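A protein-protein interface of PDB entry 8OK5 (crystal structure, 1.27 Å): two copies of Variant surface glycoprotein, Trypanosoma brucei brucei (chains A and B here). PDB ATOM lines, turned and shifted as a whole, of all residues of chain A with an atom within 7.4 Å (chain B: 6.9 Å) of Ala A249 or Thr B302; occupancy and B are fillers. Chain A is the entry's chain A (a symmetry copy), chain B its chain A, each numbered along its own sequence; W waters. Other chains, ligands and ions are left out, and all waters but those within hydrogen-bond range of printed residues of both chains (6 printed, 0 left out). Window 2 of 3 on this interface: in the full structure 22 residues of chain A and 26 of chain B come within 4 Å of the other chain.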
ATOM      1  N   THR A  27      14.626  14.405 -10.974  1.00  0.00           N
ATOM      2  CA  THR A  27      13.904  13.274 -10.364  1.00  0.00           C
ATOM      3  C   THR A  27      14.610  11.948 -10.627  1.00  0.00           C
ATOM      4  O   THR A  27      14.933  11.657 -11.775  1.00  0.00           O
ATOM      5  CB  THR A  27      12.444  13.266 -10.829  1.00  0.00           C
ATOM      6  OG1 THR A  27      11.884  14.532 -10.505  1.00  0.00           O
ATOM      7  CG2 THR A  27      11.642  12.171 -10.167  1.00  0.00           C
ATOM      8  N   GLY A  28      14.895  11.218  -9.561  1.00  0.00           N
ATOM      9  CA  GLY A  28      15.400   9.836  -9.675  1.00  0.00           C
ATOM     10  C   GLY A  28      16.879   9.707  -9.937  1.00  0.00           C
ATOM     11  O   GLY A  28      17.327   8.605 -10.042  1.00  0.00           O
ATOM     12  N   VAL A  31      18.606   7.431  -7.376  1.00  0.00           N
ATOM     13  CA  VAL A  31      18.049   6.132  -6.999  1.00  0.00           C
ATOM     14  C   VAL A  31      19.155   5.111  -6.742  1.00  0.00           C
ATOM     15  O   VAL A  31      19.048   4.299  -5.803  1.00  0.00           O
ATOM     16  CB  VAL A  31      17.031   5.645  -8.048  1.00  0.00           C
ATOM     17  CG1 VAL A  31      16.621   4.192  -7.808  1.00  0.00           C
ATOM     18  CG2 VAL A  31      15.808   6.602  -8.018  1.00  0.00           C
ATOM     19  N   ARG A  34      20.673   5.942  -3.319  1.00  0.00           N
ATOM     20  CA  ARG A  34      19.689   5.686  -2.280  1.00  0.00           C
ATOM     21  C   ARG A  34      19.613   4.200  -1.988  1.00  0.00           C
ATOM     22  O   ARG A  34      19.627   3.781  -0.809  1.00  0.00           O
ATOM     23  CB  ARG A  34      18.332   6.224  -2.685  1.00  0.00           C
ATOM     24  CG  ARG A  34      17.239   6.018  -1.649  1.00  0.00           C
ATOM     25  CD  ARG A  34      15.866   5.921  -2.244  1.00  0.00           C
ATOM     26  NE  ARG A  34      15.721   4.674  -2.961  1.00  0.00           N
ATOM     27  CZ  ARG A  34      14.986   4.493  -4.054  1.00  0.00           C
ATOM     28  NH1 ARG A  34      14.427   5.516  -4.670  1.00  0.00           N
ATOM     29  NH2 ARG A  34      14.815   3.285  -4.545  1.00  0.00           N
ATOM     30  N   LYS A 245      14.111  16.063  -5.744  1.00  0.00           N
ATOM     31  CA  LYS A 245      13.408  14.800  -6.096  1.00  0.00           C
ATOM     32  C   LYS A 245      14.422  13.722  -6.498  1.00  0.00           C
ATOM     33  O   LYS A 245      13.989  12.727  -7.023  1.00  0.00           O
ATOM     34  CB  LYS A 245      12.376  15.080  -7.194  1.00  0.00           C
ATOM     35  CG  LYS A 245      11.192  15.916  -6.736  1.00  0.00           C
ATOM     36  CD  LYS A 245      10.140  16.090  -7.796  1.00  0.00           C
ATOM     37  CE  LYS A 245       8.883  16.716  -7.235  1.00  0.00           C
ATOM     38  NZ  LYS A 245       8.007  17.242  -8.309  1.00  0.00           N
ATOM     39  N   ALA A 246      15.717  13.891  -6.248  1.00  0.00           N
ATOM     40  CA  ALA A 246      16.750  12.944  -6.745  1.00  0.00           C
ATOM     41  C   ALA A 246      16.510  11.516  -6.238  1.00  0.00           C
ATOM     42  O   ALA A 246      16.718  10.623  -6.986  1.00  0.00           O
ATOM     43  CB  ALA A 246      18.121  13.426  -6.360  1.00  0.00           C
ATOM     44  N   CYS A 247      15.974  11.332  -5.044  1.00  0.00           N
ATOM     45  CA  CYS A 247      15.827   9.958  -4.477  1.00  0.00           C
ATOM     46  C   CYS A 247      14.385   9.475  -4.564  1.00  0.00           C
ATOM     47  O   CYS A 247      14.141   8.436  -4.029  1.00  0.00           O
ATOM     48  CB  CYS A 247      16.299   9.977  -3.035  1.00  0.00           C
ATOM     49  SG  CYS A 247      18.074  10.335  -2.922  1.00  0.00           S
ATOM     50  N   VAL A 248      13.467  10.240  -5.157  1.00  0.00           N
ATOM     51  CA  VAL A 248      12.062   9.849  -5.122  1.00  0.00           C
ATOM     52  C   VAL A 248      11.470   9.714  -6.511  1.00  0.00           C
ATOM     53  O   VAL A 248      12.187   9.805  -7.523  1.00  0.00           O
ATOM     54  CB  VAL A 248      11.249  10.824  -4.243  1.00  0.00           C
ATOM     55  CG1 VAL A 248      11.758  10.780  -2.799  1.00  0.00           C
ATOM     56  CG2 VAL A 248      11.349  12.240  -4.837  1.00  0.00           C
ATOM     57  N   ALA A 249      10.171   9.462  -6.559  1.00  0.00           N
ATOM     58  CA  ALA A 249       9.403   9.431  -7.808  1.00  0.00           C
ATOM     59  C   ALA A 249       8.693  10.770  -7.966  1.00  0.00           C
ATOM     60  O   ALA A 249       9.326  11.778  -8.274  1.00  0.00           O
ATOM     61  CB  ALA A 249       8.461   8.238  -7.795  1.00  0.00           C
ATOM     62  N   GLY A 250       7.393  10.793  -7.712  1.00  0.00           N
ATOM     63  CA  GLY A 250       6.592  11.958  -8.002  1.00  0.00           C
ATOM     64  C   GLY A 250       6.761  13.120  -7.046  1.00  0.00           C
ATOM     65  O   GLY A 250       6.870  14.270  -7.485  1.00  0.00           O
ATOM     66  N   THR A 251       6.787  12.842  -5.747  1.00  0.00           N
ATOM     67  CA  THR A 251       6.638  13.874  -4.726  1.00  0.00           C
ATOM     68  C   THR A 251       7.904  13.967  -3.879  1.00  0.00           C
ATOM     69  O   THR A 251       8.390  12.961  -3.376  1.00  0.00           O
ATOM     70  CB  THR A 251       5.438  13.568  -3.824  1.00  0.00           C
ATOM     71  OG1 THR A 251       4.262  13.314  -4.618  1.00  0.00           O
ATOM     72  CG2 THR A 251       5.169  14.716  -2.865  1.00  0.00           C
ATOM     73  N   ALA A 252       8.407  15.189  -3.691  1.00  0.00           N
ATOM     74  CA  ALA A 252       9.632  15.398  -2.919  1.00  0.00           C
ATOM     75  C   ALA A 252       9.414  15.011  -1.463  1.00  0.00           C
ATOM     76  O   ALA A 252       8.285  15.046  -0.970  1.00  0.00           O
ATOM     77  CB  ALA A 252      10.057  16.872  -2.993  1.00  0.00           C
ATOM     78  N   LEU A 276      12.381   6.456   3.240  1.00  0.00           N
ATOM     79  CA  LEU A 276      12.632   5.875   1.908  1.00  0.00           C
ATOM     80  C   LEU A 276      13.243   4.483   2.004  1.00  0.00           C
ATOM     81  O   LEU A 276      13.245   3.723   1.010  1.00  0.00           O
ATOM     82  CB  LEU A 276      13.589   6.766   1.134  1.00  0.00           C
ATOM     83  CG  LEU A 276      13.079   8.184   0.821  1.00  0.00           C
ATOM     84  CD1 LEU A 276      14.162   8.970   0.171  1.00  0.00           C
ATOM     85  CD2 LEU A 276      11.826   8.082  -0.056  1.00  0.00           C
ATOM     86  N   HIS B  33      17.463  -1.021 -13.550  1.00  0.00           N
ATOM     87  CA  HIS B  33      16.321  -1.852 -13.196  1.00  0.00           C
ATOM     88  C   HIS B  33      16.275  -3.112 -14.037  1.00  0.00           C
ATOM     89  O   HIS B  33      15.956  -4.180 -13.514  1.00  0.00           O
ATOM     90  CB  HIS B  33      15.030  -1.043 -13.342  1.00  0.00           C
ATOM     91  CG  HIS B  33      15.127   0.343 -12.819  1.00  0.00           C
ATOM     92  ND1 HIS B  33      15.645   1.360 -13.583  1.00  0.00           N
ATOM     93  CD2 HIS B  33      14.813   0.885 -11.622  1.00  0.00           C
ATOM     94  CE1 HIS B  33      15.624   2.470 -12.879  1.00  0.00           C
ATOM     95  NE2 HIS B  33      15.137   2.217 -11.687  1.00  0.00           N
ATOM     96  N   ALA B 216       1.323   6.346  -9.080  1.00  0.00           N
ATOM     97  CA  ALA B 216       1.530   6.871  -7.737  1.00  0.00           C
ATOM     98  C   ALA B 216       0.420   6.509  -6.776  1.00  0.00           C
ATOM     99  O   ALA B 216       0.614   6.689  -5.585  1.00  0.00           O
ATOM    100  CB  ALA B 216       1.668   8.391  -7.831  1.00  0.00           C
ATOM    101  N   VAL B 297      16.685  -5.942  -6.317  1.00  0.00           N
ATOM    102  CA  VAL B 297      15.388  -5.461  -6.725  1.00  0.00           C
ATOM    103  C   VAL B 297      14.726  -4.668  -5.608  1.00  0.00           C
ATOM    104  O   VAL B 297      14.197  -3.566  -5.853  1.00  0.00           O
ATOM    105  CB  VAL B 297      14.487  -6.637  -7.172  1.00  0.00           C
ATOM    106  CG1 VAL B 297      13.063  -6.153  -7.437  1.00  0.00           C
ATOM    107  CG2 VAL B 297      15.085  -7.333  -8.354  1.00  0.00           C
ATOM    108  N   GLY B 298      14.728  -5.234  -4.398  1.00  0.00           N
ATOM    109  CA  GLY B 298      13.914  -4.665  -3.326  1.00  0.00           C
ATOM    110  C   GLY B 298      14.278  -3.241  -2.972  1.00  0.00           C
ATOM    111  O   GLY B 298      13.403  -2.419  -2.724  1.00  0.00           O
ATOM    112  N   ASN B 299      15.538  -2.920  -2.987  1.00  0.00           N
ATOM    113  CA  ASN B 299      15.943  -1.580  -2.605  1.00  0.00           C
ATOM    114  C   ASN B 299      15.917  -0.607  -3.763  1.00  0.00           C
ATOM    115  O   ASN B 299      16.052   0.594  -3.549  1.00  0.00           O
ATOM    116  CB  ASN B 299      17.294  -1.574  -1.934  1.00  0.00           C
ATOM    117  CG  ASN B 299      17.200  -2.088  -0.494  1.00  0.00           C
ATOM    118  OD1 ASN B 299      16.161  -1.897   0.157  1.00  0.00           O
ATOM    119  ND2 ASN B 299      18.242  -2.748  -0.021  1.00  0.00           N
ATOM    120  N   LEU B 300      15.637  -1.079  -4.974  1.00  0.00           N
ATOM    121  CA  LEU B 300      15.344  -0.183  -6.076  1.00  0.00           C
ATOM    122  C   LEU B 300      13.921   0.318  -6.010  1.00  0.00           C
ATOM    123  O   LEU B 300      13.595   1.297  -6.680  1.00  0.00           O
ATOM    124  CB  LEU B 300      15.572  -0.829  -7.463  1.00  0.00           C
ATOM    125  CG  LEU B 300      17.023  -1.032  -7.830  1.00  0.00           C
ATOM    126  CD1 LEU B 300      17.068  -1.848  -9.131  1.00  0.00           C
ATOM    127  CD2 LEU B 300      17.763   0.255  -8.011  1.00  0.00           C
ATOM    128  N   LEU B 301      13.063  -0.356  -5.245  1.00  0.00           N
ATOM    129  CA  LEU B 301      11.684   0.137  -5.087  1.00  0.00           C
ATOM    130  C   LEU B 301      11.697   1.505  -4.424  1.00  0.00           C
ATOM    131  O   LEU B 301      12.183   1.670  -3.309  1.00  0.00           O
ATOM    132  CB  LEU B 301      10.883  -0.844  -4.230  1.00  0.00           C
ATOM    133  CG  LEU B 301      10.520  -2.149  -4.936  1.00  0.00           C
ATOM    134  CD1 LEU B 301      10.117  -3.243  -3.943  1.00  0.00           C
ATOM    135  CD2 LEU B 301       9.400  -1.922  -5.928  1.00  0.00           C
ATOM    136  N   THR B 302      11.167   2.482  -5.131  1.00  0.00           N
ATOM    137  CA  THR B 302      11.104   3.863  -4.656  1.00  0.00           C
ATOM    138  C   THR B 302       9.833   4.049  -3.854  1.00  0.00           C
ATOM    139  O   THR B 302       8.734   4.023  -4.414  1.00  0.00           O
ATOM    140  CB  THR B 302      11.154   4.836  -5.838  1.00  0.00           C
ATOM    141  OG1 THR B 302      12.403   4.619  -6.509  1.00  0.00           O
ATOM    142  CG2 THR B 302      11.075   6.304  -5.331  1.00  0.00           C
ATOM    143  N   ARG B 303       9.966   4.182  -2.543  1.00  0.00           N
ATOM    144  CA  ARG B 303       8.818   4.106  -1.656  1.00  0.00           C
ATOM    145  C   ARG B 303       8.140   5.464  -1.557  1.00  0.00           C
ATOM    146  O   ARG B 303       8.751   6.442  -1.134  1.00  0.00           O
ATOM    147  CB  ARG B 303       9.256   3.626  -0.272  1.00  0.00           C
ATOM    148  CG  ARG B 303       9.656   2.152  -0.230  1.00  0.00           C
ATOM    149  CD  ARG B 303      10.306   1.741   1.059  1.00  0.00           C
ATOM    150  NE  ARG B 303      10.618   0.322   1.114  1.00  0.00           N
ATOM    151  CZ  ARG B 303       9.915  -0.600   1.765  1.00  0.00           C
ATOM    152  NH1 ARG B 303       8.868  -0.287   2.526  1.00  0.00           N
ATOM    153  NH2 ARG B 303      10.302  -1.863   1.691  1.00  0.00           N
ATOM    154  N   GLY B 304       6.867   5.491  -1.931  1.00  0.00           N
ATOM    155  CA  GLY B 304       6.027   6.655  -1.785  1.00  0.00           C
ATOM    156  C   GLY B 304       4.893   6.457  -0.790  1.00  0.00           C
ATOM    157  O   GLY B 304       4.854   5.500  -0.021  1.00  0.00           O
ATOM    158  N   SER B 305       3.992   7.425  -0.780  1.00  0.00           N
ATOM    159  CA  SER B 305       2.910   7.439   0.198  1.00  0.00           C
ATOM    160  C   SER B 305       1.893   6.340  -0.040  1.00  0.00           C
ATOM    161  O   SER B 305       1.308   5.827   0.925  1.00  0.00           O
ATOM    162  CB  SER B 305       2.213   8.809   0.160  1.00  0.00           C
ATOM    163  OG  SER B 305       1.647   9.048  -1.109  1.00  0.00           O
ATOM    164  N   THR B 307       2.247   3.919  -3.098  1.00  0.00           N
ATOM    165  CA  THR B 307       2.828   2.820  -3.842  1.00  0.00           C
ATOM    166  C   THR B 307       4.336   2.979  -3.782  1.00  0.00           C
ATOM    167  O   THR B 307       4.868   4.032  -3.410  1.00  0.00           O
ATOM    168  CB  THR B 307       2.409   2.800  -5.312  1.00  0.00           C
ATOM    169  OG1 THR B 307       2.911   3.968  -5.965  1.00  0.00           O
ATOM    170  CG2 THR B 307       0.884   2.733  -5.459  1.00  0.00           C
ATOM    171  N   SER B 308       5.029   1.910  -4.134  1.00  0.00           N
ATOM    172  CA  SER B 308       6.445   1.973  -4.438  1.00  0.00           C
ATOM    173  C   SER B 308       6.637   1.643  -5.910  1.00  0.00           C
ATOM    174  O   SER B 308       5.939   0.802  -6.480  1.00  0.00           O
ATOM    175  CB  SER B 308       7.235   1.003  -3.561  1.00  0.00           C
ATOM    176  OG  SER B 308       7.071   1.380  -2.214  1.00  0.00           O
ATOM    177  N   ILE B 309       7.609   2.278  -6.529  1.00  0.00           N
ATOM    178  CA  ILE B 309       7.805   2.241  -7.968  1.00  0.00           C
ATOM    179  C   ILE B 309       9.160   1.606  -8.269  1.00  0.00           C
ATOM    180  O   ILE B 309      10.191   2.024  -7.722  1.00  0.00           O
ATOM    181  CB  ILE B 309       7.737   3.668  -8.540  1.00  0.00           C
ATOM    182  CG1 ILE B 309       6.421   4.331  -8.190  1.00  0.00           C
ATOM    183  CG2 ILE B 309       7.959   3.625 -10.081  1.00  0.00           C
ATOM    184  CD1 ILE B 309       5.264   3.753  -8.838  1.00  0.00           C
ATOM    185  N   LEU B 310       9.154   0.683  -9.212  1.00  0.00           N
ATOM    186  CA  LEU B 310      10.363   0.093  -9.780  1.00  0.00           C
ATOM    187  C   LEU B 310      10.495   0.571 -11.224  1.00  0.00           C
ATOM    188  O   LEU B 310       9.652   0.256 -12.071  1.00  0.00           O
ATOM    189  CB  LEU B 310      10.311  -1.445  -9.705  1.00  0.00           C
ATOM    190  CG  LEU B 310      11.478  -2.207 -10.322  1.00  0.00           C
ATOM    191  CD1 LEU B 310      12.774  -1.880  -9.553  1.00  0.00           C
ATOM    192  CD2 LEU B 310      11.219  -3.708 -10.336  1.00  0.00           C
ATOM    193  N   GLY B 311      11.549   1.312 -11.525  1.00  0.00           N
ATOM    194  CA  GLY B 311      11.745   1.892 -12.847  1.00  0.00           C
ATOM    195  C   GLY B 311      11.727   3.422 -12.797  1.00  0.00           C
ATOM    196  O   GLY B 311      11.282   4.045 -11.829  1.00  0.00           O
ATOM    197  N   PHE B 313      10.604   7.036 -13.152  1.00  0.00           N
ATOM    198  CA  PHE B 313       9.289   7.657 -12.961  1.00  0.00           C
ATOM    199  C   PHE B 313       9.511   9.149 -12.801  1.00  0.00           C
ATOM    200  O   PHE B 313      10.305   9.546 -11.931  1.00  0.00           O
ATOM    201  CB  PHE B 313       8.642   7.112 -11.696  1.00  0.00           C
ATOM    202  CG  PHE B 313       7.270   7.688 -11.375  1.00  0.00           C
ATOM    203  CD1 PHE B 313       7.117   8.966 -10.855  1.00  0.00           C
ATOM    204  CD2 PHE B 313       6.156   6.939 -11.590  1.00  0.00           C
ATOM    205  CE1 PHE B 313       5.849   9.446 -10.529  1.00  0.00           C
ATOM    206  CE2 PHE B 313       4.890   7.416 -11.253  1.00  0.00           C
ATOM    207  CZ  PHE B 313       4.751   8.671 -10.744  1.00  0.00           C
ATOM    208  N   LEU B 314       8.812   9.943 -13.589  1.00  0.00           N
ATOM    209  CA  LEU B 314       8.825  11.401 -13.527  1.00  0.00           C
ATOM    210  C   LEU B 314       7.525  11.970 -13.013  1.00  0.00           C
ATOM    211  O   LEU B 314       7.544  12.886 -12.190  1.00  0.00           O
ATOM    212  CB  LEU B 314       9.131  12.003 -14.895  1.00  0.00           C
ATOM    213  CG  LEU B 314      10.511  11.692 -15.480  1.00  0.00           C
ATOM    214  CD1 LEU B 314      10.682  12.461 -16.772  1.00  0.00           C
ATOM    215  CD2 LEU B 314      11.643  12.023 -14.524  1.00  0.00           C
ATOM    216  N   ALA B 315       6.375  11.481 -13.459  1.00  0.00           N
ATOM    217  CA  ALA B 315       5.120  12.079 -13.042  1.00  0.00           C
ATOM    218  C   ALA B 315       3.947  11.140 -13.266  1.00  0.00           C
ATOM    219  O   ALA B 315       3.870  10.473 -14.300  1.00  0.00           O
ATOM    220  CB  ALA B 315       4.868  13.351 -13.845  1.00  0.00           C
ATOM    221  N   VAL B 333       4.179  -2.449  -0.607  1.00  0.00           N
ATOM    222  CA  VAL B 333       5.168  -1.752   0.195  1.00  0.00           C
ATOM    223  C   VAL B 333       5.087  -0.262  -0.136  1.00  0.00           C
ATOM    224  O   VAL B 333       4.822   0.126  -1.284  1.00  0.00           O
ATOM    225  CB  VAL B 333       6.594  -2.322  -0.010  1.00  0.00           C
ATOM    226  CG1 VAL B 333       6.592  -3.846   0.121  1.00  0.00           C
ATOM    227  CG2 VAL B 333       7.173  -1.907  -1.322  1.00  0.00           C
ATOM    228  N   THR B 334       5.274   0.562   0.888  1.00  0.00           N
ATOM    229  CA  THR B 334       5.220   2.011   0.758  1.00  0.00           C
ATOM    230  C   THR B 334       6.256   2.601   1.714  1.00  0.00           C
ATOM    231  O   THR B 334       7.009   1.876   2.375  1.00  0.00           O
ATOM    232  CB  THR B 334       3.831   2.515   1.174  1.00  0.00           C
ATOM    233  OG1 THR B 334       3.673   2.277   2.581  1.00  0.00           O
ATOM    234  CG2 THR B 334       2.698   1.812   0.436  1.00  0.00           C
ATOM    235  N   ASP B 335       6.219   3.926   1.878  1.00  0.00           N
ATOM    236  CA  ASP B 335       7.122   4.556   2.828  1.00  0.00           C
ATOM    237  C   ASP B 335       6.667   4.385   4.272  1.00  0.00           C
ATOM    238  O   ASP B 335       7.308   4.927   5.176  1.00  0.00           O
ATOM    239  CB  ASP B 335       7.348   6.032   2.462  1.00  0.00           C
ATOM    240  CG  ASP B 335       6.084   6.911   2.588  1.00  0.00           C
ATOM    241  OD1 ASP B 335       5.117   6.517   3.269  1.00  0.00           O
ATOM    242  OD2 ASP B 335       6.116   8.061   2.060  1.00  0.00           O
HETATM  243  O   HOH W   1      11.940   8.124  -9.723  1.00  0.00           O
HETATM  244  O   HOH W   2      14.511   1.153   0.335  1.00  0.00           O
HETATM  245  O   HOH W   3      12.673   4.096  -1.652  1.00  0.00           O
HETATM  246  O   HOH W   4       5.760  14.555 -10.406  1.00  0.00           O
HETATM  247  O   HOH W   5       9.470  14.791 -11.704  1.00  0.00           O
HETATM  248  O   HOH W   6      16.245   2.275  -1.485  1.00  0.00           O
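O of Asn B299 sits at hydrogen-bond distance from NH2 of Arg A34. The backbone carbonyl oxygen of Leu B300 lies within hydrogen-bond range of the guanidinium group of Arg A34, 3.2 Å away. O of Leu B301 is in hydrogen-bond range of NH2 of Arg A34 (3.3 Å). OG1 of Thr B302 lies within hydrogen-bond range of NH1 of Arg A34, at 2.9 Å.
The backbone NH of Thr B302 lies within hydrogen-bond range of the backbone carbonyl oxygen of Ile B309 (2.8 Å). The guanidinium group (NH1) of Arg B303 lies within hydrogen-bond range of the backbone carbonyl oxygen (O) of Thr B334 (2.9 Å). The guanidinium group of Arg A34 is in hydrogen-bond range of the backbone carbonyl oxygen of Cys A247, 3.0 Å away. NZ of Lys A245 sits close to O of Gly A250 (3.3 Å).
Among the printed residues, merely in contact across the chains: Ala A249 with Phe B313 (3.4 Å), Thr A27 with Phe B313 (3.4 Å), Gly A250 with Phe B313 (3.5 Å), Ala A249 with Thr B302 (3.5 Å), Leu A276 with Arg B303 (3.5 Å), Val A248 with Thr B302 (3.6 Å), Cys A247 with Thr B302 (3.95 Å) and Thr A27 with Leu B314 (3.98 Å).
Of the printed residues of chain B, Val A248 touches Thr B302. Of the printed residues of chain B, Ala A249 touches Thr B302 and Phe B313. Gly B298 touches none of the printed residues of chain A. Of the printed residues of chain A, Leu B301 touches Arg A34. Of the printed residues of chain A, Thr B302 touches Arg A34 (2.9 Å), Cys A247 (3.95 Å), Val A248 (3.6 Å) and Ala A249 (3.5 Å). Ile B309 touches none of the printed residues of chain A. The nearest printed residue of chain A that does not touch Thr B302 is Val A31 (4.2 Å). The nearest printed residue of chain B that does not touch Thr A27 is Ala B315 (6.2 Å).
Hydrophobic or aromatic side chains of chain B that line the printed part of chain A: Phe B313 and Leu B314. Along chain B the printed residues that touch a printed residue of chain A span positions 299 to 314. Of the 13 printed residues of chain A, 7 touch a printed residue of chain B. Hydrophobic or aromatic side chains of chain A that line the printed part of chain B: Ala A249 and Leu A276. Among the printed residues, no Asp or Glu carboxylate lies within 4 Å of a Lys or Arg side-chain nitrogen of the other chain.
No position is printed for both chains. Of the 12 pairs that touch across the chains among the printed residues, none has its exchanged pair printed and touching as well.
Water W6 lies within hydrogen-bond range of the backbone carbonyl oxygen of Asn B299 (2.7 Å) and the guanidinium group of Arg A34 (2.9 Å). Water W5 bridges OG1 of Thr A27 and O of Leu B314. Water W3 lies within hydrogen-bond range of the backbone carbonyl oxygen of Leu A276 (2.7 Å), the backbone NH of Arg B303 (2.9 Å), the backbone carbonyl oxygen of Leu B301 (3.0 Å) and the guanidinium group of Arg A34 (3.4 Å). Water W1 bridges the backbone carbonyl oxygen (O) of Val A248 (2.8 Å) and the backbone carbonyl oxygen (O) of Phe B313 (3.1 Å). Water W2 bridges O of Leu A276 (2.9 Å) and OD1 of Asn B299 (3.5 Å). Water W4 lies within hydrogen-bond range of O of Leu B314 and O of Gly A250.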
